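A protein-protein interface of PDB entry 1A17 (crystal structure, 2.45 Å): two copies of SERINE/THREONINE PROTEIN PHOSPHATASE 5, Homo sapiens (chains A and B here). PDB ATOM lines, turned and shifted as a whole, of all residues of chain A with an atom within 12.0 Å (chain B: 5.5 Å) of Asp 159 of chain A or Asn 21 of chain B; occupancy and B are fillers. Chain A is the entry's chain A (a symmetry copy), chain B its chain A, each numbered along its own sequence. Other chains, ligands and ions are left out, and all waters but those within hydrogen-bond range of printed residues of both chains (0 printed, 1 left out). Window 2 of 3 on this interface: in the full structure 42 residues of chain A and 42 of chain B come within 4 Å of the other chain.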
ATOM      1  N   GLU A 153      23.556  19.711 -21.686  1.00  0.00           N
ATOM      2  CA  GLU A 153      24.198  18.845 -20.690  1.00  0.00           C
ATOM      3  C   GLU A 153      23.622  18.879 -19.265  1.00  0.00           C
ATOM      4  O   GLU A 153      23.639  17.879 -18.574  1.00  0.00           O
ATOM      5  CB  GLU A 153      25.705  19.122 -20.656  1.00  0.00           C
ATOM      6  CG  GLU A 153      26.527  17.979 -20.068  1.00  0.00           C
ATOM      7  CD  GLU A 153      26.145  16.607 -20.653  1.00  0.00           C
ATOM      8  OE1 GLU A 153      26.468  16.366 -21.842  1.00  0.00           O
ATOM      9  OE2 GLU A 153      25.512  15.785 -19.930  1.00  0.00           O
ATOM     10  N   SER A 154      23.127  20.022 -18.819  1.00  0.00           N
ATOM     11  CA  SER A 154      22.567  20.115 -17.478  1.00  0.00           C
ATOM     12  C   SER A 154      21.114  19.730 -17.447  1.00  0.00           C
ATOM     13  O   SER A 154      20.477  19.799 -16.394  1.00  0.00           O
ATOM     14  CB  SER A 154      22.700  21.524 -16.895  1.00  0.00           C
ATOM     15  OG  SER A 154      24.054  21.865 -16.626  1.00  0.00           O
ATOM     16  N   MET A 155      20.549  19.431 -18.609  1.00  0.00           N
ATOM     17  CA  MET A 155      19.153  19.027 -18.637  1.00  0.00           C
ATOM     18  C   MET A 155      19.094  17.619 -18.059  1.00  0.00           C
ATOM     19  O   MET A 155      20.082  16.883 -18.131  1.00  0.00           O
ATOM     20  CB  MET A 155      18.611  19.078 -20.061  1.00  0.00           C
ATOM     21  CG  MET A 155      18.553  20.491 -20.575  1.00  0.00           C
ATOM     22  SD  MET A 155      17.869  20.748 -22.214  1.00  0.00           S
ATOM     23  CE  MET A 155      18.006  22.555 -22.261  1.00  0.00           C
ATOM     24  N   THR A 156      17.957  17.252 -17.474  1.00  0.00           N
ATOM     25  CA  THR A 156      17.800  15.929 -16.868  1.00  0.00           C
ATOM     26  C   THR A 156      16.608  15.102 -17.295  1.00  0.00           C
ATOM     27  O   THR A 156      15.478  15.578 -17.453  1.00  0.00           O
ATOM     28  CB  THR A 156      17.763  15.983 -15.341  1.00  0.00           C
ATOM     29  OG1 THR A 156      16.848  16.999 -14.929  1.00  0.00           O
ATOM     30  CG2 THR A 156      19.149  16.256 -14.781  1.00  0.00           C
ATOM     31  N   ILE A 157      16.895  13.817 -17.427  1.00  0.00           N
ATOM     32  CA  ILE A 157      15.920  12.824 -17.804  1.00  0.00           C
ATOM     33  C   ILE A 157      15.042  12.710 -16.570  1.00  0.00           C
ATOM     34  O   ILE A 157      15.459  13.068 -15.455  1.00  0.00           O
ATOM     35  CB  ILE A 157      16.664  11.512 -18.179  1.00  0.00           C
ATOM     36  CG1 ILE A 157      16.026  10.903 -19.411  1.00  0.00           C
ATOM     37  CG2 ILE A 157      16.847  10.564 -16.981  1.00  0.00           C
ATOM     38  CD1 ILE A 157      16.216  11.746 -20.644  1.00  0.00           C
ATOM     39  N   GLU A 158      13.792  12.333 -16.759  1.00  0.00           N
ATOM     40  CA  GLU A 158      12.940  12.225 -15.594  1.00  0.00           C
ATOM     41  C   GLU A 158      13.395  11.056 -14.729  1.00  0.00           C
ATOM     42  O   GLU A 158      13.186   9.901 -15.088  1.00  0.00           O
ATOM     43  CB  GLU A 158      11.470  12.057 -15.987  1.00  0.00           C
ATOM     44  CG  GLU A 158      10.508  12.113 -14.792  1.00  0.00           C
ATOM     45  CD  GLU A 158      10.518  13.463 -14.081  1.00  0.00           C
ATOM     46  OE1 GLU A 158       9.716  14.333 -14.486  1.00  0.00           O
ATOM     47  OE2 GLU A 158      11.326  13.649 -13.130  1.00  0.00           O
ATOM     48  N   ASP A 159      14.090  11.345 -13.633  1.00  0.00           N
ATOM     49  CA  ASP A 159      14.530  10.274 -12.740  1.00  0.00           C
ATOM     50  C   ASP A 159      13.563  10.174 -11.558  1.00  0.00           C
ATOM     51  O   ASP A 159      13.873  10.572 -10.428  1.00  0.00           O
ATOM     52  CB  ASP A 159      15.997  10.457 -12.296  1.00  0.00           C
ATOM     53  CG  ASP A 159      16.947   9.434 -12.954  1.00  0.00           C
ATOM     54  OD1 ASP A 159      16.555   8.248 -13.070  1.00  0.00           O
ATOM     55  OD2 ASP A 159      18.082   9.811 -13.352  1.00  0.00           O
ATOM     56  N   GLU A 160      12.365   9.687 -11.882  1.00  0.00           N
ATOM     57  CA  GLU A 160      11.243   9.471 -10.961  1.00  0.00           C
ATOM     58  C   GLU A 160      10.319   8.478 -11.695  1.00  0.00           C
ATOM     59  O   GLU A 160      10.334   8.447 -12.932  1.00  0.00           O
ATOM     60  CB  GLU A 160      10.515  10.797 -10.686  1.00  0.00           C
ATOM     61  CG  GLU A 160      11.115  11.603  -9.523  1.00  0.00           C
ATOM     62  CD  GLU A 160      11.010  13.105  -9.722  1.00  0.00           C
ATOM     63  OE1 GLU A 160       9.883  13.649  -9.620  1.00  0.00           O
ATOM     64  OE2 GLU A 160      12.061  13.739  -9.980  1.00  0.00           O
ATOM     65  N   TYR A 161       9.584   7.633 -10.961  1.00  0.00           N
ATOM     66  CA  TYR A 161       8.674   6.632 -11.579  1.00  0.00           C
ATOM     67  C   TYR A 161       7.691   7.266 -12.604  1.00  0.00           C
ATOM     68  O   TYR A 161       7.291   8.435 -12.456  1.00  0.00           O
ATOM     69  CB  TYR A 161       7.924   5.817 -10.479  1.00  0.00           C
ATOM     70  CG  TYR A 161       6.837   4.808 -10.934  1.00  0.00           C
ATOM     71  CD1 TYR A 161       7.163   3.584 -11.530  1.00  0.00           C
ATOM     72  CD2 TYR A 161       5.488   5.067 -10.700  1.00  0.00           C
ATOM     73  CE1 TYR A 161       6.169   2.652 -11.875  1.00  0.00           C
ATOM     74  CE2 TYR A 161       4.495   4.150 -11.038  1.00  0.00           C
ATOM     75  CZ  TYR A 161       4.834   2.943 -11.624  1.00  0.00           C
ATOM     76  OH  TYR A 161       3.818   2.046 -11.948  1.00  0.00           O
ATOM     77  N   SER A 162       7.366   6.509 -13.659  1.00  0.00           N
ATOM     78  CA  SER A 162       6.449   6.964 -14.710  1.00  0.00           C
ATOM     79  C   SER A 162       5.698   5.803 -15.372  1.00  0.00           C
ATOM     80  O   SER A 162       5.420   4.764 -14.751  1.00  0.00           O
ATOM     81  CB  SER A 162       7.210   7.758 -15.776  1.00  0.00           C
ATOM     82  OG  SER A 162       8.011   6.914 -16.573  1.00  0.00           O
ATOM     83  N   LEU B  16      12.096  -1.260 -19.696  1.00  0.00           N
ATOM     84  CA  LEU B  16      12.790  -0.731 -20.866  1.00  0.00           C
ATOM     85  C   LEU B  16      13.134   0.741 -20.644  1.00  0.00           C
ATOM     86  O   LEU B  16      14.238   1.164 -20.975  1.00  0.00           O
ATOM     87  CB  LEU B  16      11.945  -0.921 -22.120  1.00  0.00           C
ATOM     88  CG  LEU B  16      11.911  -2.388 -22.525  1.00  0.00           C
ATOM     89  CD1 LEU B  16      10.839  -2.616 -23.554  1.00  0.00           C
ATOM     90  CD2 LEU B  16      13.274  -2.800 -23.045  1.00  0.00           C
ATOM     91  N   LYS B  17      12.215   1.494 -20.032  1.00  0.00           N
ATOM     92  CA  LYS B  17      12.447   2.906 -19.726  1.00  0.00           C
ATOM     93  C   LYS B  17      13.662   3.004 -18.827  1.00  0.00           C
ATOM     94  O   LYS B  17      14.526   3.838 -19.058  1.00  0.00           O
ATOM     95  CB  LYS B  17      11.260   3.526 -19.005  1.00  0.00           C
ATOM     96  CG  LYS B  17      11.443   5.011 -18.714  1.00  0.00           C
ATOM     97  CD  LYS B  17      11.000   5.371 -17.308  1.00  0.00           C
ATOM     98  CE  LYS B  17      11.938   4.763 -16.295  1.00  0.00           C
ATOM     99  NZ  LYS B  17      11.402   4.844 -14.919  1.00  0.00           N
ATOM    100  N   THR B  18      13.744   2.141 -17.816  1.00  0.00           N
ATOM    101  CA  THR B  18      14.879   2.132 -16.903  1.00  0.00           C
ATOM    102  C   THR B  18      16.141   1.747 -17.648  1.00  0.00           C
ATOM    103  O   THR B  18      17.187   2.387 -17.457  1.00  0.00           O
ATOM    104  CB  THR B  18      14.642   1.200 -15.722  1.00  0.00           C
ATOM    105  OG1 THR B  18      13.663   1.793 -14.857  1.00  0.00           O
ATOM    106  CG2 THR B  18      15.922   0.991 -14.937  1.00  0.00           C
ATOM    107  N   GLN B  19      16.036   0.733 -18.520  1.00  0.00           N
ATOM    108  CA  GLN B  19      17.168   0.288 -19.333  1.00  0.00           C
ATOM    109  C   GLN B  19      17.709   1.490 -20.115  1.00  0.00           C
ATOM    110  O   GLN B  19      18.922   1.748 -20.136  1.00  0.00           O
ATOM    111  CB  GLN B  19      16.748  -0.814 -20.310  1.00  0.00           C
ATOM    112  CG  GLN B  19      16.639  -2.213 -19.684  1.00  0.00           C
ATOM    113  CD  GLN B  19      16.710  -3.345 -20.714  1.00  0.00           C
ATOM    114  OE1 GLN B  19      15.767  -4.144 -20.848  1.00  0.00           O
ATOM    115  NE2 GLN B  19      17.825  -3.428 -21.437  1.00  0.00           N
ATOM    116  N   ALA B  20      16.784   2.247 -20.707  1.00  0.00           N
ATOM    117  CA  ALA B  20      17.098   3.428 -21.478  1.00  0.00           C
ATOM    118  C   ALA B  20      17.801   4.453 -20.596  1.00  0.00           C
ATOM    119  O   ALA B  20      18.835   4.988 -20.995  1.00  0.00           O
ATOM    120  CB  ALA B  20      15.846   4.003 -22.047  1.00  0.00           C
ATOM    121  N   ASN B  21      17.274   4.700 -19.394  1.00  0.00           N
ATOM    122  CA  ASN B  21      17.872   5.678 -18.474  1.00  0.00           C
ATOM    123  C   ASN B  21      19.303   5.332 -18.161  1.00  0.00           C
ATOM    124  O   ASN B  21      20.161   6.208 -18.034  1.00  0.00           O
ATOM    125  CB  ASN B  21      17.124   5.766 -17.151  1.00  0.00           C
ATOM    126  CG  ASN B  21      15.806   6.473 -17.269  1.00  0.00           C
ATOM    127  OD1 ASN B  21      15.448   6.972 -18.336  1.00  0.00           O
ATOM    128  ND2 ASN B  21      15.060   6.510 -16.168  1.00  0.00           N
ATOM    129  N   ASP B  22      19.547   4.051 -17.970  1.00  0.00           N
ATOM    130  CA  ASP B  22      20.875   3.613 -17.680  1.00  0.00           C
ATOM    131  C   ASP B  22      21.729   4.046 -18.829  1.00  0.00           C
ATOM    132  O   ASP B  22      22.700   4.776 -18.648  1.00  0.00           O
ATOM    133  CB  ASP B  22      20.889   2.105 -17.561  1.00  0.00           C
ATOM    134  CG  ASP B  22      20.306   1.631 -16.259  1.00  0.00           C
ATOM    135  OD1 ASP B  22      19.924   2.483 -15.411  1.00  0.00           O
ATOM    136  OD2 ASP B  22      20.247   0.393 -16.083  1.00  0.00           O
ATOM    137  N   TYR B  23      21.333   3.627 -20.027  1.00  0.00           N
ATOM    138  CA  TYR B  23      22.074   3.966 -21.229  1.00  0.00           C
ATOM    139  C   TYR B  23      22.229   5.484 -21.369  1.00  0.00           C
ATOM    140  O   TYR B  23      23.273   5.973 -21.801  1.00  0.00           O
ATOM    141  CB  TYR B  23      21.406   3.347 -22.456  1.00  0.00           C
ATOM    142  CG  TYR B  23      21.741   1.865 -22.691  1.00  0.00           C
ATOM    143  CD1 TYR B  23      23.064   1.449 -22.914  1.00  0.00           C
ATOM    144  CD2 TYR B  23      20.728   0.889 -22.759  1.00  0.00           C
ATOM    145  CE1 TYR B  23      23.368   0.098 -23.212  1.00  0.00           C
ATOM    146  CE2 TYR B  23      21.024  -0.463 -23.055  1.00  0.00           C
ATOM    147  CZ  TYR B  23      22.343  -0.850 -23.284  1.00  0.00           C
ATOM    148  OH  TYR B  23      22.654  -2.166 -23.584  1.00  0.00           O
ATOM    149  N   PHE B  24      21.226   6.231 -20.940  1.00  0.00           N
ATOM    150  CA  PHE B  24      21.293   7.691 -21.012  1.00  0.00           C
ATOM    151  C   PHE B  24      22.384   8.247 -20.087  1.00  0.00           C
ATOM    152  O   PHE B  24      23.276   8.970 -20.534  1.00  0.00           O
ATOM    153  CB  PHE B  24      19.939   8.321 -20.651  1.00  0.00           C
ATOM    154  CG  PHE B  24      19.897   9.814 -20.820  1.00  0.00           C
ATOM    155  CD1 PHE B  24      20.269  10.655 -19.780  1.00  0.00           C
ATOM    156  CD2 PHE B  24      19.477  10.383 -22.024  1.00  0.00           C
ATOM    157  CE1 PHE B  24      20.226  12.036 -19.929  1.00  0.00           C
ATOM    158  CE2 PHE B  24      19.427  11.768 -22.187  1.00  0.00           C
ATOM    159  CZ  PHE B  24      19.802  12.596 -21.137  1.00  0.00           C
ATOM    160  N   LYS B  25      22.310   7.918 -18.797  1.00  0.00           N
ATOM    161  CA  LYS B  25      23.289   8.392 -17.839  1.00  0.00           C
ATOM    162  C   LYS B  25      24.723   7.961 -18.150  1.00  0.00           C
ATOM    163  O   LYS B  25      25.675   8.598 -17.692  1.00  0.00           O
ATOM    164  CB  LYS B  25      22.854   8.042 -16.420  1.00  0.00           C
ATOM    165  CG  LYS B  25      21.713   8.965 -15.952  1.00  0.00           C
ATOM    166  CD  LYS B  25      21.088   8.566 -14.622  1.00  0.00           C
ATOM    167  CE  LYS B  25      20.269   7.302 -14.749  1.00  0.00           C
ATOM    168  NZ  LYS B  25      19.491   7.016 -13.512  1.00  0.00           N
ATOM    169  N   ALA B  26      24.864   6.938 -18.995  1.00  0.00           N
ATOM    170  CA  ALA B  26      26.162   6.428 -19.432  1.00  0.00           C
ATOM    171  C   ALA B  26      26.562   6.988 -20.817  1.00  0.00           C
ATOM    172  O   ALA B  26      27.440   6.448 -21.502  1.00  0.00           O
ATOM    173  CB  ALA B  26      26.144   4.910 -19.453  1.00  0.00           C
ATOM    174  N   TYR B  36      13.787   3.958 -25.278  1.00  0.00           N
ATOM    175  CA  TYR B  36      12.612   4.772 -24.954  1.00  0.00           C
ATOM    176  C   TYR B  36      11.590   4.426 -25.999  1.00  0.00           C
ATOM    177  O   TYR B  36      10.419   4.367 -25.695  1.00  0.00           O
ATOM    178  CB  TYR B  36      12.875   6.254 -25.031  1.00  0.00           C
ATOM    179  CG  TYR B  36      13.728   6.740 -23.908  1.00  0.00           C
ATOM    180  CD1 TYR B  36      13.407   6.450 -22.587  1.00  0.00           C
ATOM    181  CD2 TYR B  36      14.856   7.491 -24.161  1.00  0.00           C
ATOM    182  CE1 TYR B  36      14.201   6.912 -21.546  1.00  0.00           C
ATOM    183  CE2 TYR B  36      15.655   7.951 -23.132  1.00  0.00           C
ATOM    184  CZ  TYR B  36      15.324   7.662 -21.839  1.00  0.00           C
ATOM    185  OH  TYR B  36      16.123   8.142 -20.854  1.00  0.00           O
ATOM    186  N   ASN B  52      11.595  12.040 -22.104  1.00  0.00           N
ATOM    187  CA  ASN B  52      12.938  11.524 -22.029  1.00  0.00           C
ATOM    188  C   ASN B  52      13.570  11.364 -23.377  1.00  0.00           C
ATOM    189  O   ASN B  52      14.711  11.781 -23.574  1.00  0.00           O
ATOM    190  CB  ASN B  52      12.949  10.200 -21.282  1.00  0.00           C
ATOM    191  CG  ASN B  52      12.694  10.374 -19.808  1.00  0.00           C
ATOM    192  OD1 ASN B  52      12.641  11.499 -19.296  1.00  0.00           O
ATOM    193  ND2 ASN B  52      12.561   9.264 -19.106  1.00  0.00           N
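Hydrophobic or aromatic side chains of chain A within 4 Å of the printed part of chain B: Ile 157.
Hydrophobic or aromatic side chains of chain B within 4 Å of the printed part of chain A: Phe 24 and Tyr 36.
The side-chain amide oxygen (OD1) of Asn 52 of chain B lies within hydrogen-bond range of the backbone NH (N) of Glu 158 of chain A, at 2.9 Å.
The side-chain amino group (NZ) of Lys 25 of chain B lies within salt-bridge range of the side-chain carboxylate (OD2) of Asp 159 of chain A (3.1 Å).
Phe 24 of chain B touches Ile 157 of chain A (CE2 to CD1, 3.6 Å).
OH of Tyr 36 of chain B touches CG1 of Ile 157 of chain A (3.1 Å).
Ile 157 of chain A touches Asn 52 of chain B (CD1 to O, 3.3 Å).
Asn 21 of chain B touches Asp 159 of chain A (ND2 to OD1, 3.9 Å).
Lys 17 of chain B touches Ser 162 of chain A (CD to OG, 3.4 Å).
The side-chain hydroxyl (OH) of Tyr 36 of chain B sits at hydrogen-bond distance from the side-chain amide oxygen (OD1) of Asn 21 of chain B (2.9 Å).
The side-chain amide oxygen (OD1) of Asn 21 of chain B sits close to the backbone carbonyl oxygen (O) of Lys 17 of chain B (3.3 Å).
Asp 159 of chain A touches just these residues of chain B: Asn 21 and Lys 25.
Of the printed residues of chain A, Asn 21 of chain B touches Asp 159 (3.9 Å).
Lys 17 of chain B touches just one residue of chain A: Ser 162.
No residue of chain A comes within 4 Å of Thr 18 of chain B.
No residue of chain A comes within 4 Å of Ala 20 of chain B.
Printed residues of chain A within 4 Å of Phe 24 of chain B: Ile 157.
Lys 25 of chain B touches one residue of chain A.
Of chain A, only Ile 157 (3.3 Å) and Glu 158 (2.9 Å) come within 4 Å of Asn 52 of chain B.
Of the printed residues of chain B, Ser 162 of chain A touches Lys 17.
Of the printed residues of chain B, Ile 157 of chain A touches Phe 24 (3.6 Å), Tyr 36 (3.1 Å) and Asn 52 (3.3 Å).
Printed residues of chain B within 4 Å of Glu 158 of chain A: Asn 52 (2.9 Å).
No position is printed for both chains.
Of the 7 pairs that touch across the chains among the printed residues, none has its exchanged pair printed and touching as well.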
